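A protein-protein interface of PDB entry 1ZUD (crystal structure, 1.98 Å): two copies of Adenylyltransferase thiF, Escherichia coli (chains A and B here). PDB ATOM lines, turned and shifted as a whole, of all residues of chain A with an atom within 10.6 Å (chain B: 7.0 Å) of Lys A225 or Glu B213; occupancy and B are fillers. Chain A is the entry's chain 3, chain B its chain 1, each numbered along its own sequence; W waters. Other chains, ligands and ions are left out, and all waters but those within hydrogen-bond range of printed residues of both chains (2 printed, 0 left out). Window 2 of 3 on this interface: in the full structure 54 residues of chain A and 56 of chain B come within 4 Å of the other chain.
The side-chain carboxylate (OE1) of Glu B204 is in hydrogen-bond range of the side-chain hydroxyl (OG) of Ser A227, at 3.2 Å.
The backbone carbonyl oxygen of Gly A224 lies within hydrogen-bond range of the side-chain amino group of Lys B207.
OG of Ser A227 is in hydrogen-bond range of NZ of Lys B207, 3.0 Å away.
The side-chain amino group (NZ) of Lys A225 is in salt-bridge range of the side-chain carboxylate (OE2) of Glu B213, 3.8 Å away.
The side-chain hydroxyl (OG1) of Thr B214 lies within hydrogen-bond range of the backbone carbonyl oxygen (O) of Lys A225.
NZ of Lys B207 is in salt-bridge range of OE1 of Glu B204, 3.0 Å away.
O of Lys B207 lies within hydrogen-bond range of N of Ile B212 (2.8 Å).
O of Phe A154 sits at hydrogen-bond distance from N of Gly A224, 2.7 Å away.
The backbone NH (N) of Phe A222 lies within hydrogen-bond range of the backbone carbonyl oxygen (O) of Gly A156 (2.8 Å).
The side-chain carboxylate (OD1) of Asp A223 sits at hydrogen-bond distance from the backbone NH (N) of Ser A226 (3.0 Å).
OG of Ser A226 lies close to N of Gln A228 (3.4 Å).
Val A190 touches Leu B203 (CG1 to CD1, 3.8 Å).
Pro A192 touches Leu B203 (CB to CB, 3.8 Å).
Leu B203 touches Val A193 (CD1 to CG2, 3.8 Å).
Phe A222 touches Leu B203.
CD2 of Leu B203 touches O of Gly A224 (3.8 Å).
Lys A225 touches Lys B207.
CG of Lys A225 touches CG2 of Ile B212 (3.7 Å).
Lys A225 touches Pro B215 (O to CD, 3.7 Å).
Ser A226 touches Pro B215 (O to CG, 3.5 Å).
Thr B214 touches Ser A227.
Lys A225 touches just these residues of chain B: Asp B17, Lys B207, Ile B212, Glu B213, Thr B214 and Pro B215.
Of the printed residues of chain B, Ser A226 touches Pro B215 (3.5 Å).
Gln A228 touches none of the printed residues of chain B.
Of the printed residues of chain A, Asp B17 touches Lys A225 (3.9 Å).
Printed residues of chain A within 4 Å of Leu B203: Val A190 (3.8 Å), Pro A192 (3.8 Å), Val A193 (3.8 Å), Phe A222 (3.9 Å) and Gly A224 (3.8 Å).
Printed residues of chain A within 4 Å of Lys B207: Gly A224 (2.9 Å), Lys A225 (3.7 Å) and Ser A227 (3.0 Å).
Ser B210 touches none of the printed residues of chain A.
Gly B211 touches none of the printed residues of chain A.
Of chain A, only Lys A225 (3.8 Å) comes within 4 Å of Glu B213.
Thr B214 touches just these residues of chain A: Lys A225 (2.6 Å) and Ser A227 (3.6 Å).
Of the printed residues of chain A, Pro B215 touches Lys A225 (3.7 Å) and Ser A226 (3.5 Å).
The nearest residue of chain B that does not touch Lys A225 is Leu B203 (5.7 Å).
Hydrophobic or aromatic side chains of chain A that line the printed part of chain B: Phe A154, Val A190, Pro A192, Val A193 and Phe A222.
Hydrophobic or aromatic side chains of chain B within 4 Å of the printed part of chain A: Leu B203, Ile B212 and Pro B215.
Among the printed residues, Asp or Glu carboxylates within 4 Å of a Lys or Arg side-chain nitrogen of the other chain: Lys A225 with Glu B213 (3.8 Å).
No position is printed for both chains.
Water W2 lies within hydrogen-bond range of the backbone carbonyl oxygen of Pro B215, the side-chain carboxylate of Glu B204, the side-chain hydroxyl of Ser A227 and the side-chain hydroxyl of Thr B214.
Water W1 lies within hydrogen-bond range of the side-chain carboxylate (OE1) of Glu B204 (2.8 Å), the side-chain hydroxyl (OG) of Ser A227 (2.8 Å), the backbone carbonyl oxygen (O) of Gly A224 (3.0 Å) and the side-chain amino group (NZ) of Lys B207 (3.3 Å).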
ATOM      1  N   VAL A 152      18.778 -22.118 -23.452  1.00  0.00           N
ATOM      2  CA  VAL A 152      17.957 -23.291 -23.750  1.00  0.00           C
ATOM      3  C   VAL A 152      16.549 -22.842 -23.427  1.00  0.00           C
ATOM      4  O   VAL A 152      16.354 -22.074 -22.491  1.00  0.00           O
ATOM      5  CB  VAL A 152      18.363 -24.600 -22.901  1.00  0.00           C
ATOM      6  CG1 VAL A 152      17.950 -24.497 -21.440  1.00  0.00           C
ATOM      7  CG2 VAL A 152      17.694 -25.837 -23.500  1.00  0.00           C
ATOM      8  N   GLY A 153      15.552 -23.278 -24.207  1.00  0.00           N
ATOM      9  CA  GLY A 153      14.196 -22.866 -23.903  1.00  0.00           C
ATOM     10  C   GLY A 153      14.081 -21.357 -23.946  1.00  0.00           C
ATOM     11  O   GLY A 153      14.426 -20.733 -24.943  1.00  0.00           O
ATOM     12  N   PHE A 154      13.577 -20.745 -22.869  1.00  0.00           N
ATOM     13  CA  PHE A 154      13.506 -19.294 -22.826  1.00  0.00           C
ATOM     14  C   PHE A 154      14.609 -18.722 -21.906  1.00  0.00           C
ATOM     15  O   PHE A 154      14.596 -17.532 -21.587  1.00  0.00           O
ATOM     16  CB  PHE A 154      12.135 -18.842 -22.281  1.00  0.00           C
ATOM     17  CG  PHE A 154      11.011 -18.945 -23.294  1.00  0.00           C
ATOM     18  CD1 PHE A 154      10.628 -17.834 -24.046  1.00  0.00           C
ATOM     19  CD2 PHE A 154      10.351 -20.159 -23.494  1.00  0.00           C
ATOM     20  CE1 PHE A 154       9.571 -17.929 -25.004  1.00  0.00           C
ATOM     21  CE2 PHE A 154       9.298 -20.268 -24.446  1.00  0.00           C
ATOM     22  CZ  PHE A 154       8.918 -19.159 -25.187  1.00  0.00           C
ATOM     23  N   GLY A 155      15.550 -19.554 -21.463  1.00  0.00           N
ATOM     24  CA  GLY A 155      16.555 -19.031 -20.550  1.00  0.00           C
ATOM     25  C   GLY A 155      17.965 -18.877 -21.080  1.00  0.00           C
ATOM     26  O   GLY A 155      18.348 -19.570 -22.030  1.00  0.00           O
ATOM     27  N   GLY A 156      18.720 -17.946 -20.466  1.00  0.00           N
ATOM     28  CA  GLY A 156      20.097 -17.678 -20.883  1.00  0.00           C
ATOM     29  C   GLY A 156      20.989 -17.414 -19.675  1.00  0.00           C
ATOM     30  O   GLY A 156      20.470 -16.980 -18.647  1.00  0.00           O
ATOM     31  N   VAL A 190      14.263 -20.859 -28.215  1.00  0.00           N
ATOM     32  CA  VAL A 190      13.690 -19.720 -28.927  1.00  0.00           C
ATOM     33  C   VAL A 190      14.857 -18.957 -29.564  1.00  0.00           C
ATOM     34  O   VAL A 190      15.866 -18.636 -28.903  1.00  0.00           O
ATOM     35  CB  VAL A 190      12.907 -18.832 -27.926  1.00  0.00           C
ATOM     36  CG1 VAL A 190      12.290 -17.648 -28.640  1.00  0.00           C
ATOM     37  CG2 VAL A 190      11.806 -19.685 -27.253  1.00  0.00           C
ATOM     38  N   PRO A 192      15.466 -15.804 -30.738  1.00  0.00           N
ATOM     39  CA  PRO A 192      15.941 -14.550 -30.153  1.00  0.00           C
ATOM     40  C   PRO A 192      16.479 -14.692 -28.739  1.00  0.00           C
ATOM     41  O   PRO A 192      17.161 -13.821 -28.280  1.00  0.00           O
ATOM     42  CB  PRO A 192      14.704 -13.641 -30.176  1.00  0.00           C
ATOM     43  CG  PRO A 192      13.769 -14.256 -31.196  1.00  0.00           C
ATOM     44  CD  PRO A 192      14.046 -15.729 -31.164  1.00  0.00           C
ATOM     45  N   VAL A 193      16.166 -15.749 -28.025  1.00  0.00           N
ATOM     46  CA  VAL A 193      16.778 -15.848 -26.683  1.00  0.00           C
ATOM     47  C   VAL A 193      18.271 -16.217 -26.822  1.00  0.00           C
ATOM     48  O   VAL A 193      19.152 -15.593 -26.218  1.00  0.00           O
ATOM     49  CB  VAL A 193      16.059 -16.907 -25.805  1.00  0.00           C
ATOM     50  CG1 VAL A 193      16.833 -17.070 -24.464  1.00  0.00           C
ATOM     51  CG2 VAL A 193      14.601 -16.459 -25.540  1.00  0.00           C
ATOM     52  N   VAL A 194      18.587 -17.237 -27.610  1.00  0.00           N
ATOM     53  CA  VAL A 194      19.990 -17.601 -27.759  1.00  0.00           C
ATOM     54  C   VAL A 194      20.682 -16.438 -28.507  1.00  0.00           C
ATOM     55  O   VAL A 194      21.862 -16.123 -28.282  1.00  0.00           O
ATOM     56  CB  VAL A 194      20.192 -18.997 -28.487  1.00  0.00           C
ATOM     57  CG1 VAL A 194      19.655 -18.985 -29.932  1.00  0.00           C
ATOM     58  CG2 VAL A 194      21.673 -19.286 -28.564  1.00  0.00           C
ATOM     59  N   VAL A 196      20.016 -13.166 -28.227  1.00  0.00           N
ATOM     60  CA  VAL A 196      20.386 -12.070 -27.371  1.00  0.00           C
ATOM     61  C   VAL A 196      21.642 -12.394 -26.544  1.00  0.00           C
ATOM     62  O   VAL A 196      22.496 -11.519 -26.368  1.00  0.00           O
ATOM     63  CB  VAL A 196      19.278 -11.596 -26.386  1.00  0.00           C
ATOM     64  CG1 VAL A 196      18.054 -11.153 -27.156  1.00  0.00           C
ATOM     65  CG2 VAL A 196      18.962 -12.615 -25.373  1.00  0.00           C
ATOM     66  N   LEU A 221      21.706 -13.871 -15.551  1.00  0.00           N
ATOM     67  CA  LEU A 221      20.711 -14.885 -15.907  1.00  0.00           C
ATOM     68  C   LEU A 221      19.496 -14.191 -16.526  1.00  0.00           C
ATOM     69  O   LEU A 221      19.002 -13.177 -16.032  1.00  0.00           O
ATOM     70  CB  LEU A 221      20.271 -15.691 -14.665  1.00  0.00           C
ATOM     71  CG  LEU A 221      21.437 -16.285 -13.812  1.00  0.00           C
ATOM     72  CD1 LEU A 221      20.857 -16.935 -12.519  1.00  0.00           C
ATOM     73  CD2 LEU A 221      22.212 -17.344 -14.575  1.00  0.00           C
ATOM     74  N   PHE A 222      19.029 -14.752 -17.622  1.00  0.00           N
ATOM     75  CA  PHE A 222      17.891 -14.152 -18.324  1.00  0.00           C
ATOM     76  C   PHE A 222      16.719 -15.138 -18.369  1.00  0.00           C
ATOM     77  O   PHE A 222      16.901 -16.293 -18.723  1.00  0.00           O
ATOM     78  CB  PHE A 222      18.346 -13.777 -19.766  1.00  0.00           C
ATOM     79  CG  PHE A 222      17.234 -13.183 -20.636  1.00  0.00           C
ATOM     80  CD1 PHE A 222      16.440 -12.152 -20.158  1.00  0.00           C
ATOM     81  CD2 PHE A 222      17.027 -13.652 -21.923  1.00  0.00           C
ATOM     82  CE1 PHE A 222      15.427 -11.564 -20.936  1.00  0.00           C
ATOM     83  CE2 PHE A 222      16.008 -13.075 -22.750  1.00  0.00           C
ATOM     84  CZ  PHE A 222      15.217 -12.040 -22.257  1.00  0.00           C
ATOM     85  N   ASP A 223      15.520 -14.692 -17.997  1.00  0.00           N
ATOM     86  CA  ASP A 223      14.315 -15.536 -18.167  1.00  0.00           C
ATOM     87  C   ASP A 223      13.521 -14.760 -19.294  1.00  0.00           C
ATOM     88  O   ASP A 223      12.917 -13.737 -19.029  1.00  0.00           O
ATOM     89  CB  ASP A 223      13.479 -15.576 -16.875  1.00  0.00           C
ATOM     90  CG  ASP A 223      12.167 -16.373 -17.039  1.00  0.00           C
ATOM     91  OD1 ASP A 223      11.652 -16.536 -18.189  1.00  0.00           O
ATOM     92  OD2 ASP A 223      11.635 -16.811 -15.999  1.00  0.00           O
ATOM     93  N   GLY A 224      13.527 -15.290 -20.519  1.00  0.00           N
ATOM     94  CA  GLY A 224      12.871 -14.644 -21.652  1.00  0.00           C
ATOM     95  C   GLY A 224      11.362 -14.654 -21.586  1.00  0.00           C
ATOM     96  O   GLY A 224      10.706 -13.948 -22.360  1.00  0.00           O
ATOM     97  N   LYS A 225      10.804 -15.473 -20.689  1.00  0.00           N
ATOM     98  CA  LYS A 225       9.349 -15.566 -20.529  1.00  0.00           C
ATOM     99  C   LYS A 225       8.844 -14.518 -19.558  1.00  0.00           C
ATOM    100  O   LYS A 225       7.816 -13.840 -19.803  1.00  0.00           O
ATOM    101  CB  LYS A 225       8.965 -16.989 -20.039  1.00  0.00           C
ATOM    102  CG  LYS A 225       7.808 -17.614 -20.796  1.00  0.00           C
ATOM    103  CD  LYS A 225       7.718 -19.121 -20.573  1.00  0.00           C
ATOM    104  CE  LYS A 225       6.839 -19.436 -19.394  1.00  0.00           C
ATOM    105  NZ  LYS A 225       5.450 -18.926 -19.607  1.00  0.00           N
ATOM    106  N   SER A 226       9.527 -14.388 -18.409  1.00  0.00           N
ATOM    107  CA  SER A 226       9.132 -13.360 -17.447  1.00  0.00           C
ATOM    108  C   SER A 226       9.785 -12.018 -17.864  1.00  0.00           C
ATOM    109  O   SER A 226       9.428 -10.962 -17.326  1.00  0.00           O
ATOM    110  CB  SER A 226       9.630 -13.719 -16.030  1.00  0.00           C
ATOM    111  OG  SER A 226      11.038 -13.572 -16.018  1.00  0.00           O
ATOM    112  N   SER A 227      10.748 -12.069 -18.791  1.00  0.00           N
ATOM    113  CA  SER A 227      11.447 -10.858 -19.275  1.00  0.00           C
ATOM    114  C   SER A 227      12.267 -10.176 -18.194  1.00  0.00           C
ATOM    115  O   SER A 227      12.379  -8.943 -18.139  1.00  0.00           O
ATOM    116  CB  SER A 227      10.443  -9.845 -19.846  1.00  0.00           C
ATOM    117  OG  SER A 227       9.791 -10.431 -20.967  1.00  0.00           O
ATOM    118  N   GLN A 228      12.831 -10.991 -17.324  1.00  0.00           N
ATOM    119  CA  GLN A 228      13.637 -10.484 -16.199  1.00  0.00           C
ATOM    120  C   GLN A 228      15.101 -10.943 -16.239  1.00  0.00           C
ATOM    121  O   GLN A 228      15.373 -12.012 -16.719  1.00  0.00           O
ATOM    122  CB  GLN A 228      13.032 -10.987 -14.900  1.00  0.00           C
ATOM    123  CG  GLN A 228      11.621 -10.453 -14.644  1.00  0.00           C
ATOM    124  CD  GLN A 228      11.104 -10.810 -13.247  1.00  0.00           C
ATOM    125  OE1 GLN A 228      10.952 -11.987 -12.900  1.00  0.00           O
ATOM    126  NE2 GLN A 228      10.840  -9.785 -12.434  1.00  0.00           N
ATOM    127  N   TRP A 229      16.014 -10.114 -15.734  1.00  0.00           N
ATOM    128  CA  TRP A 229      17.431 -10.424 -15.653  1.00  0.00           C
ATOM    129  C   TRP A 229      17.832 -10.380 -14.161  1.00  0.00           C
ATOM    130  O   TRP A 229      17.225  -9.643 -13.391  1.00  0.00           O
ATOM    131  CB  TRP A 229      18.278  -9.334 -16.321  1.00  0.00           C
ATOM    132  CG  TRP A 229      18.261  -9.422 -17.791  1.00  0.00           C
ATOM    133  CD1 TRP A 229      17.382  -8.821 -18.634  1.00  0.00           C
ATOM    134  CD2 TRP A 229      19.203 -10.114 -18.602  1.00  0.00           C
ATOM    135  NE1 TRP A 229      17.733  -9.071 -19.934  1.00  0.00           N
ATOM    136  CE2 TRP A 229      18.848  -9.873 -19.939  1.00  0.00           C
ATOM    137  CE3 TRP A 229      20.319 -10.919 -18.322  1.00  0.00           C
ATOM    138  CZ2 TRP A 229      19.573 -10.412 -21.031  1.00  0.00           C
ATOM    139  CZ3 TRP A 229      21.040 -11.451 -19.400  1.00  0.00           C
ATOM    140  CH2 TRP A 229      20.643 -11.180 -20.751  1.00  0.00           C
ATOM    141  N   ASP B  17       5.570 -24.846 -24.865  1.00  0.00           N
ATOM    142  CA  ASP B  17       4.866 -23.575 -24.924  1.00  0.00           C
ATOM    143  C   ASP B  17       4.573 -23.129 -26.358  1.00  0.00           C
ATOM    144  O   ASP B  17       3.771 -22.250 -26.547  1.00  0.00           O
ATOM    145  CB  ASP B  17       5.667 -22.464 -24.261  1.00  0.00           C
ATOM    146  CG  ASP B  17       5.658 -22.562 -22.784  1.00  0.00           C
ATOM    147  OD1 ASP B  17       4.562 -22.698 -22.200  1.00  0.00           O
ATOM    148  OD2 ASP B  17       6.751 -22.494 -22.202  1.00  0.00           O
ATOM    149  N   LEU B 203      11.702 -11.293 -29.876  1.00  0.00           N
ATOM    150  CA  LEU B 203      11.256 -12.209 -28.844  1.00  0.00           C
ATOM    151  C   LEU B 203       9.850 -11.817 -28.355  1.00  0.00           C
ATOM    152  O   LEU B 203       8.991 -12.682 -28.152  1.00  0.00           O
ATOM    153  CB  LEU B 203      12.248 -12.168 -27.654  1.00  0.00           C
ATOM    154  CG  LEU B 203      11.791 -12.955 -26.407  1.00  0.00           C
ATOM    155  CD1 LEU B 203      11.626 -14.466 -26.759  1.00  0.00           C
ATOM    156  CD2 LEU B 203      12.842 -12.821 -25.306  1.00  0.00           C
ATOM    157  N   GLU B 204       9.580 -10.530 -28.148  1.00  0.00           N
ATOM    158  CA  GLU B 204       8.266 -10.162 -27.646  1.00  0.00           C
ATOM    159  C   GLU B 204       7.150 -10.483 -28.653  1.00  0.00           C
ATOM    160  O   GLU B 204       6.023 -10.840 -28.275  1.00  0.00           O
ATOM    161  CB  GLU B 204       8.215  -8.667 -27.279  1.00  0.00           C
ATOM    162  CG  GLU B 204       9.101  -8.305 -26.074  1.00  0.00           C
ATOM    163  CD  GLU B 204       8.721  -9.147 -24.828  1.00  0.00           C
ATOM    164  OE1 GLU B 204       9.616  -9.627 -24.091  1.00  0.00           O
ATOM    165  OE2 GLU B 204       7.512  -9.334 -24.586  1.00  0.00           O
ATOM    166  N   LYS B 207       6.259 -14.235 -28.598  1.00  0.00           N
ATOM    167  CA  LYS B 207       5.450 -14.583 -27.457  1.00  0.00           C
ATOM    168  C   LYS B 207       3.988 -14.106 -27.624  1.00  0.00           C
ATOM    169  O   LYS B 207       3.032 -14.825 -27.324  1.00  0.00           O
ATOM    170  CB  LYS B 207       6.056 -13.925 -26.193  1.00  0.00           C
ATOM    171  CG  LYS B 207       7.324 -14.654 -25.745  1.00  0.00           C
ATOM    172  CD  LYS B 207       7.737 -14.147 -24.315  1.00  0.00           C
ATOM    173  CE  LYS B 207       8.381 -12.795 -24.449  1.00  0.00           C
ATOM    174  NZ  LYS B 207       8.497 -12.180 -23.091  1.00  0.00           N
ATOM    175  N   SER B 210       2.279 -16.205 -30.366  1.00  0.00           N
ATOM    176  CA  SER B 210       2.033 -17.589 -30.036  1.00  0.00           C
ATOM    177  C   SER B 210       1.168 -17.727 -28.779  1.00  0.00           C
ATOM    178  O   SER B 210       0.811 -18.831 -28.399  1.00  0.00           O
ATOM    179  CB  SER B 210       3.377 -18.361 -29.915  1.00  0.00           C
ATOM    180  OG  SER B 210       4.187 -17.830 -28.866  1.00  0.00           O
ATOM    181  N   GLY B 211       0.825 -16.623 -28.120  1.00  0.00           N
ATOM    182  CA  GLY B 211      -0.036 -16.710 -26.946  1.00  0.00           C
ATOM    183  C   GLY B 211       0.699 -17.053 -25.640  1.00  0.00           C
ATOM    184  O   GLY B 211       0.111 -17.594 -24.683  1.00  0.00           O
ATOM    185  N   ILE B 212       1.983 -16.738 -25.563  1.00  0.00           N
ATOM    186  CA  ILE B 212       2.728 -17.043 -24.339  1.00  0.00           C
ATOM    187  C   ILE B 212       2.514 -15.896 -23.358  1.00  0.00           C
ATOM    188  O   ILE B 212       2.685 -14.743 -23.701  1.00  0.00           O
ATOM    189  CB  ILE B 212       4.230 -17.277 -24.684  1.00  0.00           C
ATOM    190  CG1 ILE B 212       4.328 -18.595 -25.448  1.00  0.00           C
ATOM    191  CG2 ILE B 212       5.136 -17.335 -23.411  1.00  0.00           C
ATOM    192  CD1 ILE B 212       5.597 -18.785 -26.121  1.00  0.00           C
ATOM    193  N   GLU B 213       2.102 -16.229 -22.144  1.00  0.00           N
ATOM    194  CA  GLU B 213       1.836 -15.228 -21.110  1.00  0.00           C
ATOM    195  C   GLU B 213       3.160 -14.579 -20.741  1.00  0.00           C
ATOM    196  O   GLU B 213       4.138 -15.269 -20.413  1.00  0.00           O
ATOM    197  CB  GLU B 213       1.256 -15.896 -19.856  1.00  0.00           C
ATOM    198  CG  GLU B 213       2.125 -17.065 -19.360  1.00  0.00           C
ATOM    199  CD  GLU B 213       1.661 -18.448 -19.879  1.00  0.00           C
ATOM    200  OE1 GLU B 213       0.986 -19.156 -19.089  1.00  0.00           O
ATOM    201  OE2 GLU B 213       1.954 -18.823 -21.056  1.00  0.00           O
ATOM    202  N   THR B 214       3.185 -13.253 -20.756  1.00  0.00           N
ATOM    203  CA  THR B 214       4.411 -12.543 -20.446  1.00  0.00           C
ATOM    204  C   THR B 214       3.970 -11.142 -20.044  1.00  0.00           C
ATOM    205  O   THR B 214       2.863 -10.763 -20.312  1.00  0.00           O
ATOM    206  CB  THR B 214       5.320 -12.557 -21.737  1.00  0.00           C
ATOM    207  OG1 THR B 214       6.671 -12.175 -21.413  1.00  0.00           O
ATOM    208  CG2 THR B 214       4.714 -11.631 -22.847  1.00  0.00           C
ATOM    209  N   PRO B 215       4.822 -10.366 -19.367  1.00  0.00           N
ATOM    210  CA  PRO B 215       4.412  -9.008 -18.970  1.00  0.00           C
ATOM    211  C   PRO B 215       4.315  -8.094 -20.203  1.00  0.00           C
ATOM    212  O   PRO B 215       4.919  -8.396 -21.226  1.00  0.00           O
ATOM    213  CB  PRO B 215       5.579  -8.538 -18.089  1.00  0.00           C
ATOM    214  CG  PRO B 215       6.136  -9.831 -17.563  1.00  0.00           C
ATOM    215  CD  PRO B 215       6.122 -10.711 -18.775  1.00  0.00           C
HETATM  216  O   HOH W   1      11.623 -11.147 -22.927  1.00  0.00           O
HETATM  217  O   HOH W   2       7.280  -9.130 -21.853  1.00  0.00           O
